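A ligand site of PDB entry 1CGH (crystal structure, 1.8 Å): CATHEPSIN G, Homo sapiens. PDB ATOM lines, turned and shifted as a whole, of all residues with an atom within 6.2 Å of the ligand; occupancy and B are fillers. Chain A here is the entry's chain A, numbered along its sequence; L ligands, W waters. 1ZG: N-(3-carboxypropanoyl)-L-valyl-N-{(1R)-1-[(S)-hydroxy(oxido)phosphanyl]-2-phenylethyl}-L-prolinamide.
OG of Ser 181 is covalently linked to P of the ligand (1.6 Å). N of Ser 181 lies within hydrogen-bond range of O1P of the ligand, 3.1 Å away. N of the ligand is in hydrogen-bond range of O of Gly 198 (2.8 Å). A ring nitrogen (NE2) of His 44 lies within hydrogen-bond range of an oxygen (O2P) of the ligand, 2.8 Å away. An oxygen (O) of the ligand is in hydrogen-bond range of the backbone NH of Gly 198 (3.3 Å). The backbone NH of Asp 180 sits at hydrogen-bond distance from an oxygen (O1P) of the ligand (3.5 Å). The backbone carbonyl oxygen of Ser 196 lies within hydrogen-bond range of a nitrogen (N2) of the ligand, at 3.0 Å. The backbone NH (N) of Gly 179 lies within hydrogen-bond range of an oxygen (O1P) of the ligand (2.7 Å).
The side-chain hydroxyl (OG) of Ser 196 sits at hydrogen-bond distance from the side-chain carboxylate (OD2) of Asp 88. N of Ala 176 sits at hydrogen-bond distance from OE2 of Glu 206 (2.9 Å). OG of Ser 181 sits at hydrogen-bond distance from NE2 of His 44 (3.1 Å). The side-chain sulfur of Cys 29 is disulfide-bonded to the side-chain sulfur of Cys 45 (2.0 Å). A ring nitrogen (ND1) of His 44 is in hydrogen-bond range of the side-chain carboxylate of Asp 88. The backbone NH (N) of Phe 177 is in hydrogen-bond range of the side-chain carboxylate (OD2) of Asp 180 (2.8 Å).
CD1 of Ile 85 touches CD of the ligand, 3.9 Å away. Phe 156 touches the ligand. O of Ala 176 touches CE1 of the ligand, at 3.7 Å. Phe 177 touches the ligand (O to CB2, 3.6 Å). NZ of Lys 178 touches CG1 of the ligand (3.3 Å). Tyr 197 touches the ligand. O of Lys 199 touches CZ of the ligand, 3.3 Å away. Ser 200 touches the ligand. Glu 206 touches the ligand (OE1 to CE1, 3.5 Å). Hydrophobic or aromatic side chains that line the ligand: His 44, Ile 85, Phe 156, Phe 177 and Tyr 197. Of the 24 residues printed, 15 come within 4 Å of the ligand. The nearest printed residue that does not touch the ligand is Val 195 (4.4 Å).
Water W2 bridges the backbone NH of Ser 200 and an oxygen (O1) of the ligand. Water W1 lies within hydrogen-bond range of the backbone carbonyl oxygen of Arg 28 (2.6 Å), an oxygen (O2P) of the ligand (3.0 Å) and the side-chain sulfur of Cys 29 (3.7 Å).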
ATOM      1  N   ARG A  28      -2.920  -8.722   2.216  1.00  0.00           N
ATOM      2  CA  ARG A  28      -1.658  -8.520   2.952  1.00  0.00           C
ATOM      3  C   ARG A  28      -1.648  -7.294   3.859  1.00  0.00           C
ATOM      4  O   ARG A  28      -2.259  -6.272   3.535  1.00  0.00           O
ATOM      5  CB  ARG A  28      -0.499  -8.426   1.961  1.00  0.00           C
ATOM      6  CG  ARG A  28      -0.530  -7.179   1.060  1.00  0.00           C
ATOM      7  N   CYS A  29      -0.942  -7.375   4.981  1.00  0.00           N
ATOM      8  CA  CYS A  29      -0.830  -6.259   5.934  1.00  0.00           C
ATOM      9  C   CYS A  29       0.533  -6.315   6.605  1.00  0.00           C
ATOM     10  O   CYS A  29       1.285  -7.231   6.363  1.00  0.00           O
ATOM     11  CB  CYS A  29      -1.869  -6.395   7.034  1.00  0.00           C
ATOM     12  SG  CYS A  29      -3.552  -5.862   6.609  1.00  0.00           S
ATOM     13  N   HIS A  44      -8.790  -4.792  11.122  1.00  0.00           N
ATOM     14  CA  HIS A  44      -9.338  -4.902   9.789  1.00  0.00           C
ATOM     15  C   HIS A  44      -8.505  -5.847   8.940  1.00  0.00           C
ATOM     16  O   HIS A  44      -8.939  -6.232   7.872  1.00  0.00           O
ATOM     17  CB  HIS A  44      -9.564  -3.512   9.146  1.00  0.00           C
ATOM     18  CG  HIS A  44      -8.373  -2.909   8.458  1.00  0.00           C
ATOM     19  ND1 HIS A  44      -7.694  -1.827   8.967  1.00  0.00           N
ATOM     20  CD2 HIS A  44      -7.792  -3.190   7.263  1.00  0.00           C
ATOM     21  CE1 HIS A  44      -6.763  -1.446   8.104  1.00  0.00           C
ATOM     22  NE2 HIS A  44      -6.796  -2.262   7.059  1.00  0.00           N
ATOM     23  N   CYS A  45      -7.340  -6.265   9.438  1.00  0.00           N
ATOM     24  CA  CYS A  45      -6.487  -7.228   8.709  1.00  0.00           C
ATOM     25  C   CYS A  45      -6.835  -8.656   9.066  1.00  0.00           C
ATOM     26  O   CYS A  45      -6.142  -9.588   8.650  1.00  0.00           O
ATOM     27  CB  CYS A  45      -4.999  -7.036   9.032  1.00  0.00           C
ATOM     28  SG  CYS A  45      -4.345  -5.464   8.436  1.00  0.00           S
ATOM     29  N   ILE A  85     -14.401   1.967  11.362  1.00  0.00           N
ATOM     30  CA  ILE A  85     -12.986   1.588  11.495  1.00  0.00           C
ATOM     31  C   ILE A  85     -12.441   2.026  12.861  1.00  0.00           C
ATOM     32  O   ILE A  85     -11.284   2.442  12.996  1.00  0.00           O
ATOM     33  CB  ILE A  85     -12.135   2.188  10.343  1.00  0.00           C
ATOM     34  CG1 ILE A  85     -12.898   2.088   9.026  1.00  0.00           C
ATOM     35  CG2 ILE A  85     -10.848   1.384  10.167  1.00  0.00           C
ATOM     36  CD1 ILE A  85     -12.169   2.700   7.849  1.00  0.00           C
ATOM     37  N   ASP A  88      -9.406  -0.183  15.842  1.00  0.00           N
ATOM     38  CA  ASP A  88      -8.752  -1.032  14.824  1.00  0.00           C
ATOM     39  C   ASP A  88      -7.382  -1.562  15.328  1.00  0.00           C
ATOM     40  O   ASP A  88      -6.323  -1.064  14.996  1.00  0.00           O
ATOM     41  CB  ASP A  88      -8.616  -0.211  13.513  1.00  0.00           C
ATOM     42  CG  ASP A  88      -8.281  -1.052  12.322  1.00  0.00           C
ATOM     43  OD1 ASP A  88      -8.384  -2.299  12.363  1.00  0.00           O
ATOM     44  OD2 ASP A  88      -7.904  -0.452  11.302  1.00  0.00           O
ATOM     45  N   ILE A 155     -11.809  16.354   9.371  1.00  0.00           N
ATOM     46  CA  ILE A 155     -11.712  15.627   8.100  1.00  0.00           C
ATOM     47  C   ILE A 155     -12.381  14.254   8.027  1.00  0.00           C
ATOM     48  O   ILE A 155     -12.880  13.846   6.976  1.00  0.00           O
ATOM     49  CB  ILE A 155     -10.235  15.392   7.718  1.00  0.00           C
ATOM     50  CG1 ILE A 155      -9.429  16.676   7.883  1.00  0.00           C
ATOM     51  CG2 ILE A 155     -10.131  14.898   6.291  1.00  0.00           C
ATOM     52  CD1 ILE A 155      -7.920  16.453   8.031  1.00  0.00           C
ATOM     53  N   PHE A 156     -12.323  13.520   9.125  1.00  0.00           N
ATOM     54  CA  PHE A 156     -12.868  12.174   9.171  1.00  0.00           C
ATOM     55  C   PHE A 156     -13.998  12.136  10.197  1.00  0.00           C
ATOM     56  O   PHE A 156     -13.796  12.437  11.362  1.00  0.00           O
ATOM     57  CB  PHE A 156     -11.759  11.162   9.539  1.00  0.00           C
ATOM     58  CG  PHE A 156     -10.626  11.104   8.532  1.00  0.00           C
ATOM     59  CD1 PHE A 156     -10.795  10.480   7.290  1.00  0.00           C
ATOM     60  CD2 PHE A 156      -9.380  11.688   8.825  1.00  0.00           C
ATOM     61  CE1 PHE A 156      -9.779  10.427   6.354  1.00  0.00           C
ATOM     62  CE2 PHE A 156      -8.359  11.646   7.896  1.00  0.00           C
ATOM     63  CZ  PHE A 156      -8.551  11.024   6.663  1.00  0.00           C
ATOM     64  N   ALA A 176       1.646   6.524   4.953  1.00  0.00           N
ATOM     65  CA  ALA A 176       1.534   5.069   4.933  1.00  0.00           C
ATOM     66  C   ALA A 176       0.396   4.915   3.901  1.00  0.00           C
ATOM     67  O   ALA A 176      -0.413   5.829   3.755  1.00  0.00           O
ATOM     68  CB  ALA A 176       1.120   4.534   6.257  1.00  0.00           C
ATOM     69  N   PHE A 177       0.322   3.810   3.185  1.00  0.00           N
ATOM     70  CA  PHE A 177      -0.690   3.641   2.138  1.00  0.00           C
ATOM     71  C   PHE A 177      -1.148   2.183   2.094  1.00  0.00           C
ATOM     72  O   PHE A 177      -0.884   1.424   3.034  1.00  0.00           O
ATOM     73  CB  PHE A 177      -0.073   4.086   0.812  1.00  0.00           C
ATOM     74  CG  PHE A 177      -1.075   4.391  -0.267  1.00  0.00           C
ATOM     75  CD1 PHE A 177      -2.300   5.014   0.040  1.00  0.00           C
ATOM     76  CD2 PHE A 177      -0.801   4.036  -1.588  1.00  0.00           C
ATOM     77  CE1 PHE A 177      -3.232   5.278  -0.963  1.00  0.00           C
ATOM     78  CE2 PHE A 177      -1.710   4.295  -2.610  1.00  0.00           C
ATOM     79  CZ  PHE A 177      -2.939   4.909  -2.301  1.00  0.00           C
ATOM     80  N   LYS A 178      -1.836   1.789   1.036  1.00  0.00           N
ATOM     81  CA  LYS A 178      -2.367   0.419   0.912  1.00  0.00           C
ATOM     82  C   LYS A 178      -1.319  -0.654   1.067  1.00  0.00           C
ATOM     83  O   LYS A 178      -0.335  -0.665   0.338  1.00  0.00           O
ATOM     84  CB  LYS A 178      -3.087   0.258  -0.428  1.00  0.00           C
ATOM     85  CG  LYS A 178      -4.307   1.164  -0.524  1.00  0.00           C
ATOM     86  CD  LYS A 178      -4.853   1.300  -1.944  1.00  0.00           C
ATOM     87  CE  LYS A 178      -6.309   1.839  -1.948  1.00  0.00           C
ATOM     88  NZ  LYS A 178      -6.566   3.155  -1.208  1.00  0.00           N
ATOM     89  N   GLY A 179      -1.564  -1.580   1.991  1.00  0.00           N
ATOM     90  CA  GLY A 179      -0.594  -2.624   2.242  1.00  0.00           C
ATOM     91  C   GLY A 179       0.212  -2.357   3.497  1.00  0.00           C
ATOM     92  O   GLY A 179       0.779  -3.271   4.070  1.00  0.00           O
ATOM     93  N   ASP A 180       0.252  -1.099   3.955  1.00  0.00           N
ATOM     94  CA  ASP A 180       0.978  -0.718   5.175  1.00  0.00           C
ATOM     95  C   ASP A 180       0.152  -0.855   6.465  1.00  0.00           C
ATOM     96  O   ASP A 180       0.693  -0.735   7.564  1.00  0.00           O
ATOM     97  CB  ASP A 180       1.508   0.717   5.101  1.00  0.00           C
ATOM     98  CG  ASP A 180       2.524   0.916   3.950  1.00  0.00           C
ATOM     99  OD1 ASP A 180       3.372   0.029   3.722  1.00  0.00           O
ATOM    100  OD2 ASP A 180       2.468   1.955   3.261  1.00  0.00           O
ATOM    101  N   SER A 181      -1.155  -1.097   6.348  1.00  0.00           N
ATOM    102  CA  SER A 181      -2.009  -1.232   7.533  1.00  0.00           C
ATOM    103  C   SER A 181      -1.411  -2.227   8.519  1.00  0.00           C
ATOM    104  O   SER A 181      -0.878  -3.260   8.102  1.00  0.00           O
ATOM    105  CB  SER A 181      -3.410  -1.741   7.153  1.00  0.00           C
ATOM    106  OG  SER A 181      -4.184  -0.750   6.491  1.00  0.00           O
ATOM    107  N   GLY A 182      -1.549  -1.918   9.814  1.00  0.00           N
ATOM    108  CA  GLY A 182      -1.022  -2.775  10.850  1.00  0.00           C
ATOM    109  C   GLY A 182       0.422  -2.451  11.247  1.00  0.00           C
ATOM    110  O   GLY A 182       0.862  -2.855  12.340  1.00  0.00           O
ATOM    111  N   VAL A 195      -0.956   1.673  11.721  1.00  0.00           N
ATOM    112  CA  VAL A 195      -1.501   2.225  10.476  1.00  0.00           C
ATOM    113  C   VAL A 195      -2.924   1.689  10.344  1.00  0.00           C
ATOM    114  O   VAL A 195      -3.127   0.458  10.369  1.00  0.00           O
ATOM    115  CB  VAL A 195      -0.694   1.768   9.254  1.00  0.00           C
ATOM    116  CG1 VAL A 195      -1.396   2.234   7.950  1.00  0.00           C
ATOM    117  CG2 VAL A 195       0.717   2.338   9.333  1.00  0.00           C
ATOM    118  N   SER A 196      -3.903   2.596  10.230  1.00  0.00           N
ATOM    119  CA  SER A 196      -5.297   2.161  10.099  1.00  0.00           C
ATOM    120  C   SER A 196      -5.975   2.538   8.760  1.00  0.00           C
ATOM    121  O   SER A 196      -6.257   1.660   7.930  1.00  0.00           O
ATOM    122  CB  SER A 196      -6.113   2.692  11.287  1.00  0.00           C
ATOM    123  OG  SER A 196      -7.443   2.188  11.210  1.00  0.00           O
ATOM    124  N   TYR A 197      -6.199   3.825   8.526  1.00  0.00           N
ATOM    125  CA  TYR A 197      -6.883   4.251   7.297  1.00  0.00           C
ATOM    126  C   TYR A 197      -6.618   5.707   6.911  1.00  0.00           C
ATOM    127  O   TYR A 197      -6.033   6.479   7.682  1.00  0.00           O
ATOM    128  CB  TYR A 197      -8.414   4.035   7.463  1.00  0.00           C
ATOM    129  CG  TYR A 197      -9.135   4.993   8.404  1.00  0.00           C
ATOM    130  CD1 TYR A 197      -9.245   4.743   9.769  1.00  0.00           C
ATOM    131  CD2 TYR A 197      -9.739   6.157   7.890  1.00  0.00           C
ATOM    132  CE1 TYR A 197      -9.943   5.613  10.601  1.00  0.00           C
ATOM    133  CE2 TYR A 197     -10.446   7.027   8.711  1.00  0.00           C
ATOM    134  CZ  TYR A 197     -10.541   6.753  10.052  1.00  0.00           C
ATOM    135  OH  TYR A 197     -11.271   7.613  10.846  1.00  0.00           O
ATOM    136  N   GLY A 198      -7.093   6.078   5.733  1.00  0.00           N
ATOM    137  CA  GLY A 198      -6.939   7.445   5.268  1.00  0.00           C
ATOM    138  C   GLY A 198      -7.719   7.609   3.973  1.00  0.00           C
ATOM    139  O   GLY A 198      -8.592   6.787   3.664  1.00  0.00           O
ATOM    140  N   LYS A 199      -7.395   8.649   3.203  1.00  0.00           N
ATOM    141  CA  LYS A 199      -8.038   8.912   1.910  1.00  0.00           C
ATOM    142  C   LYS A 199      -7.523   7.988   0.820  1.00  0.00           C
ATOM    143  O   LYS A 199      -6.349   7.584   0.822  1.00  0.00           O
ATOM    144  CB  LYS A 199      -7.826  10.357   1.485  1.00  0.00           C
ATOM    145  CG  LYS A 199      -8.321  11.359   2.488  1.00  0.00           C
ATOM    146  CD  LYS A 199      -8.084  12.754   1.973  1.00  0.00           C
ATOM    147  CE  LYS A 199      -8.045  13.777   3.111  1.00  0.00           C
ATOM    148  NZ  LYS A 199      -6.789  13.740   3.984  1.00  0.00           N
ATOM    149  N   SER A 200      -8.397   7.657  -0.112  1.00  0.00           N
ATOM    150  CA  SER A 200      -8.006   6.775  -1.206  1.00  0.00           C
ATOM    151  C   SER A 200      -6.833   7.372  -2.018  1.00  0.00           C
ATOM    152  O   SER A 200      -6.061   6.644  -2.653  1.00  0.00           O
ATOM    153  CB  SER A 200      -9.222   6.523  -2.114  1.00  0.00           C
ATOM    154  OG  SER A 200      -9.200   5.201  -2.657  1.00  0.00           O
ATOM    155  N   SER A 201      -6.699   8.698  -1.978  1.00  0.00           N
ATOM    156  CA  SER A 201      -5.643   9.381  -2.713  1.00  0.00           C
ATOM    157  C   SER A 201      -4.259   9.139  -2.100  1.00  0.00           C
ATOM    158  O   SER A 201      -3.246   9.244  -2.781  1.00  0.00           O
ATOM    159  CB  SER A 201      -5.910  10.884  -2.711  1.00  0.00           C
ATOM    160  OG  SER A 201      -6.085  11.353  -1.393  1.00  0.00           O
ATOM    161  N   GLY A 202      -4.255   8.855  -0.797  1.00  0.00           N
ATOM    162  CA  GLY A 202      -3.011   8.648  -0.091  1.00  0.00           C
ATOM    163  C   GLY A 202      -2.518   9.969   0.488  1.00  0.00           C
ATOM    164  O   GLY A 202      -1.459  10.050   1.166  1.00  0.00           O
ATOM    165  N   GLU A 206      -3.739  11.149   7.816  1.00  0.00           N
ATOM    166  CA  GLU A 206      -4.339   9.822   7.845  1.00  0.00           C
ATOM    167  C   GLU A 206      -4.465   9.434   9.325  1.00  0.00           C
ATOM    168  O   GLU A 206      -3.936  10.107  10.211  1.00  0.00           O
ATOM    169  CB  GLU A 206      -3.512   8.841   7.017  1.00  0.00           C
ATOM    170  CG  GLU A 206      -2.095   8.631   7.558  1.00  0.00           C
ATOM    171  CD  GLU A 206      -1.196   7.894   6.592  1.00  0.00           C
ATOM    172  OE1 GLU A 206      -1.674   7.363   5.579  1.00  0.00           O
ATOM    173  OE2 GLU A 206       0.001   7.858   6.867  1.00  0.00           O
HETATM  174  C1  1ZG L   1     -12.243   8.941   2.915  1.00  0.00           C
HETATM  175  O1  1ZG L   1     -11.883   9.445   1.819  1.00  0.00           O
HETATM  176  O2  1ZG L   1     -12.647   9.684   4.093  1.00  0.00           O
HETATM  177  C2  1ZG L   1     -12.140   7.410   2.920  1.00  0.00           C
HETATM  178  C3  1ZG L   1     -11.728   6.782   4.282  1.00  0.00           C
HETATM  179  C4  1ZG L   1     -11.636   5.280   4.215  1.00  0.00           C
HETATM  180  O3  1ZG L   1     -12.638   4.599   4.479  1.00  0.00           O
HETATM  181  N   1ZG L   1     -10.636   4.812   3.460  1.00  0.00           N
HETATM  182  CA  1ZG L   1     -10.562   3.406   3.091  1.00  0.00           C
HETATM  183  C   1ZG L   1      -9.483   2.729   3.952  1.00  0.00           C
HETATM  184  O   1ZG L   1      -8.684   3.420   4.583  1.00  0.00           O
HETATM  185  CB  1ZG L   1     -10.290   3.207   1.533  1.00  0.00           C
HETATM  186  CG1 1ZG L   1      -8.916   3.657   1.125  1.00  0.00           C
HETATM  187  CG2 1ZG L   1     -10.443   1.779   1.168  1.00  0.00           C
HETATM  188  N1  1ZG L   1      -9.697   1.636   4.708  1.00  0.00           N
HETATM  189  CA1 1ZG L   1      -8.634   0.890   5.401  1.00  0.00           C
HETATM  190  C5  1ZG L   1      -7.419   0.617   4.514  1.00  0.00           C
HETATM  191  O4  1ZG L   1      -7.574   0.343   3.320  1.00  0.00           O
HETATM  192  CB1 1ZG L   1      -9.349  -0.386   5.873  1.00  0.00           C
HETATM  193  CG  1ZG L   1     -10.472  -0.545   4.958  1.00  0.00           C
HETATM  194  CD  1ZG L   1     -10.941   0.844   4.668  1.00  0.00           C
HETATM  195  N2  1ZG L   1      -6.210   0.718   5.103  1.00  0.00           N
HETATM  196  CA2 1ZG L   1      -5.294   0.547   4.569  1.00  0.00           C
HETATM  197  P   1ZG L   1      -4.455  -1.002   4.944  1.00  0.00           P
HETATM  198  O1P 1ZG L   1      -3.204  -1.414   4.101  1.00  0.00           O
HETATM  199  O2P 1ZG L   1      -5.376  -2.140   4.607  1.00  0.00           O
HETATM  200  CB2 1ZG L   1      -4.129   1.586   4.562  1.00  0.00           C
HETATM  201  CG3 1ZG L   1      -4.350   2.972   3.951  1.00  0.00           C
HETATM  202  CD1 1ZG L   1      -3.852   4.103   4.579  1.00  0.00           C
HETATM  203  CD2 1ZG L   1      -5.070   3.128   2.754  1.00  0.00           C
HETATM  204  CE1 1ZG L   1      -4.062   5.400   4.028  1.00  0.00           C
HETATM  205  CE2 1ZG L   1      -5.288   4.405   2.198  1.00  0.00           C
HETATM  206  CZ  1ZG L   1      -4.781   5.537   2.846  1.00  0.00           C
HETATM  207  O   HOH W   1      -3.903  -4.324   3.227  1.00  0.00           O
HETATM  208  O   HOH W   2     -10.872   8.634  -0.599  1.00  0.00           O
HETATM  209  O   HOH W   3      -7.763  -2.923   3.170  1.00  0.00           O
HETATM  210  O   HOH W   4      -6.439  -0.665   0.849  1.00  0.00           O
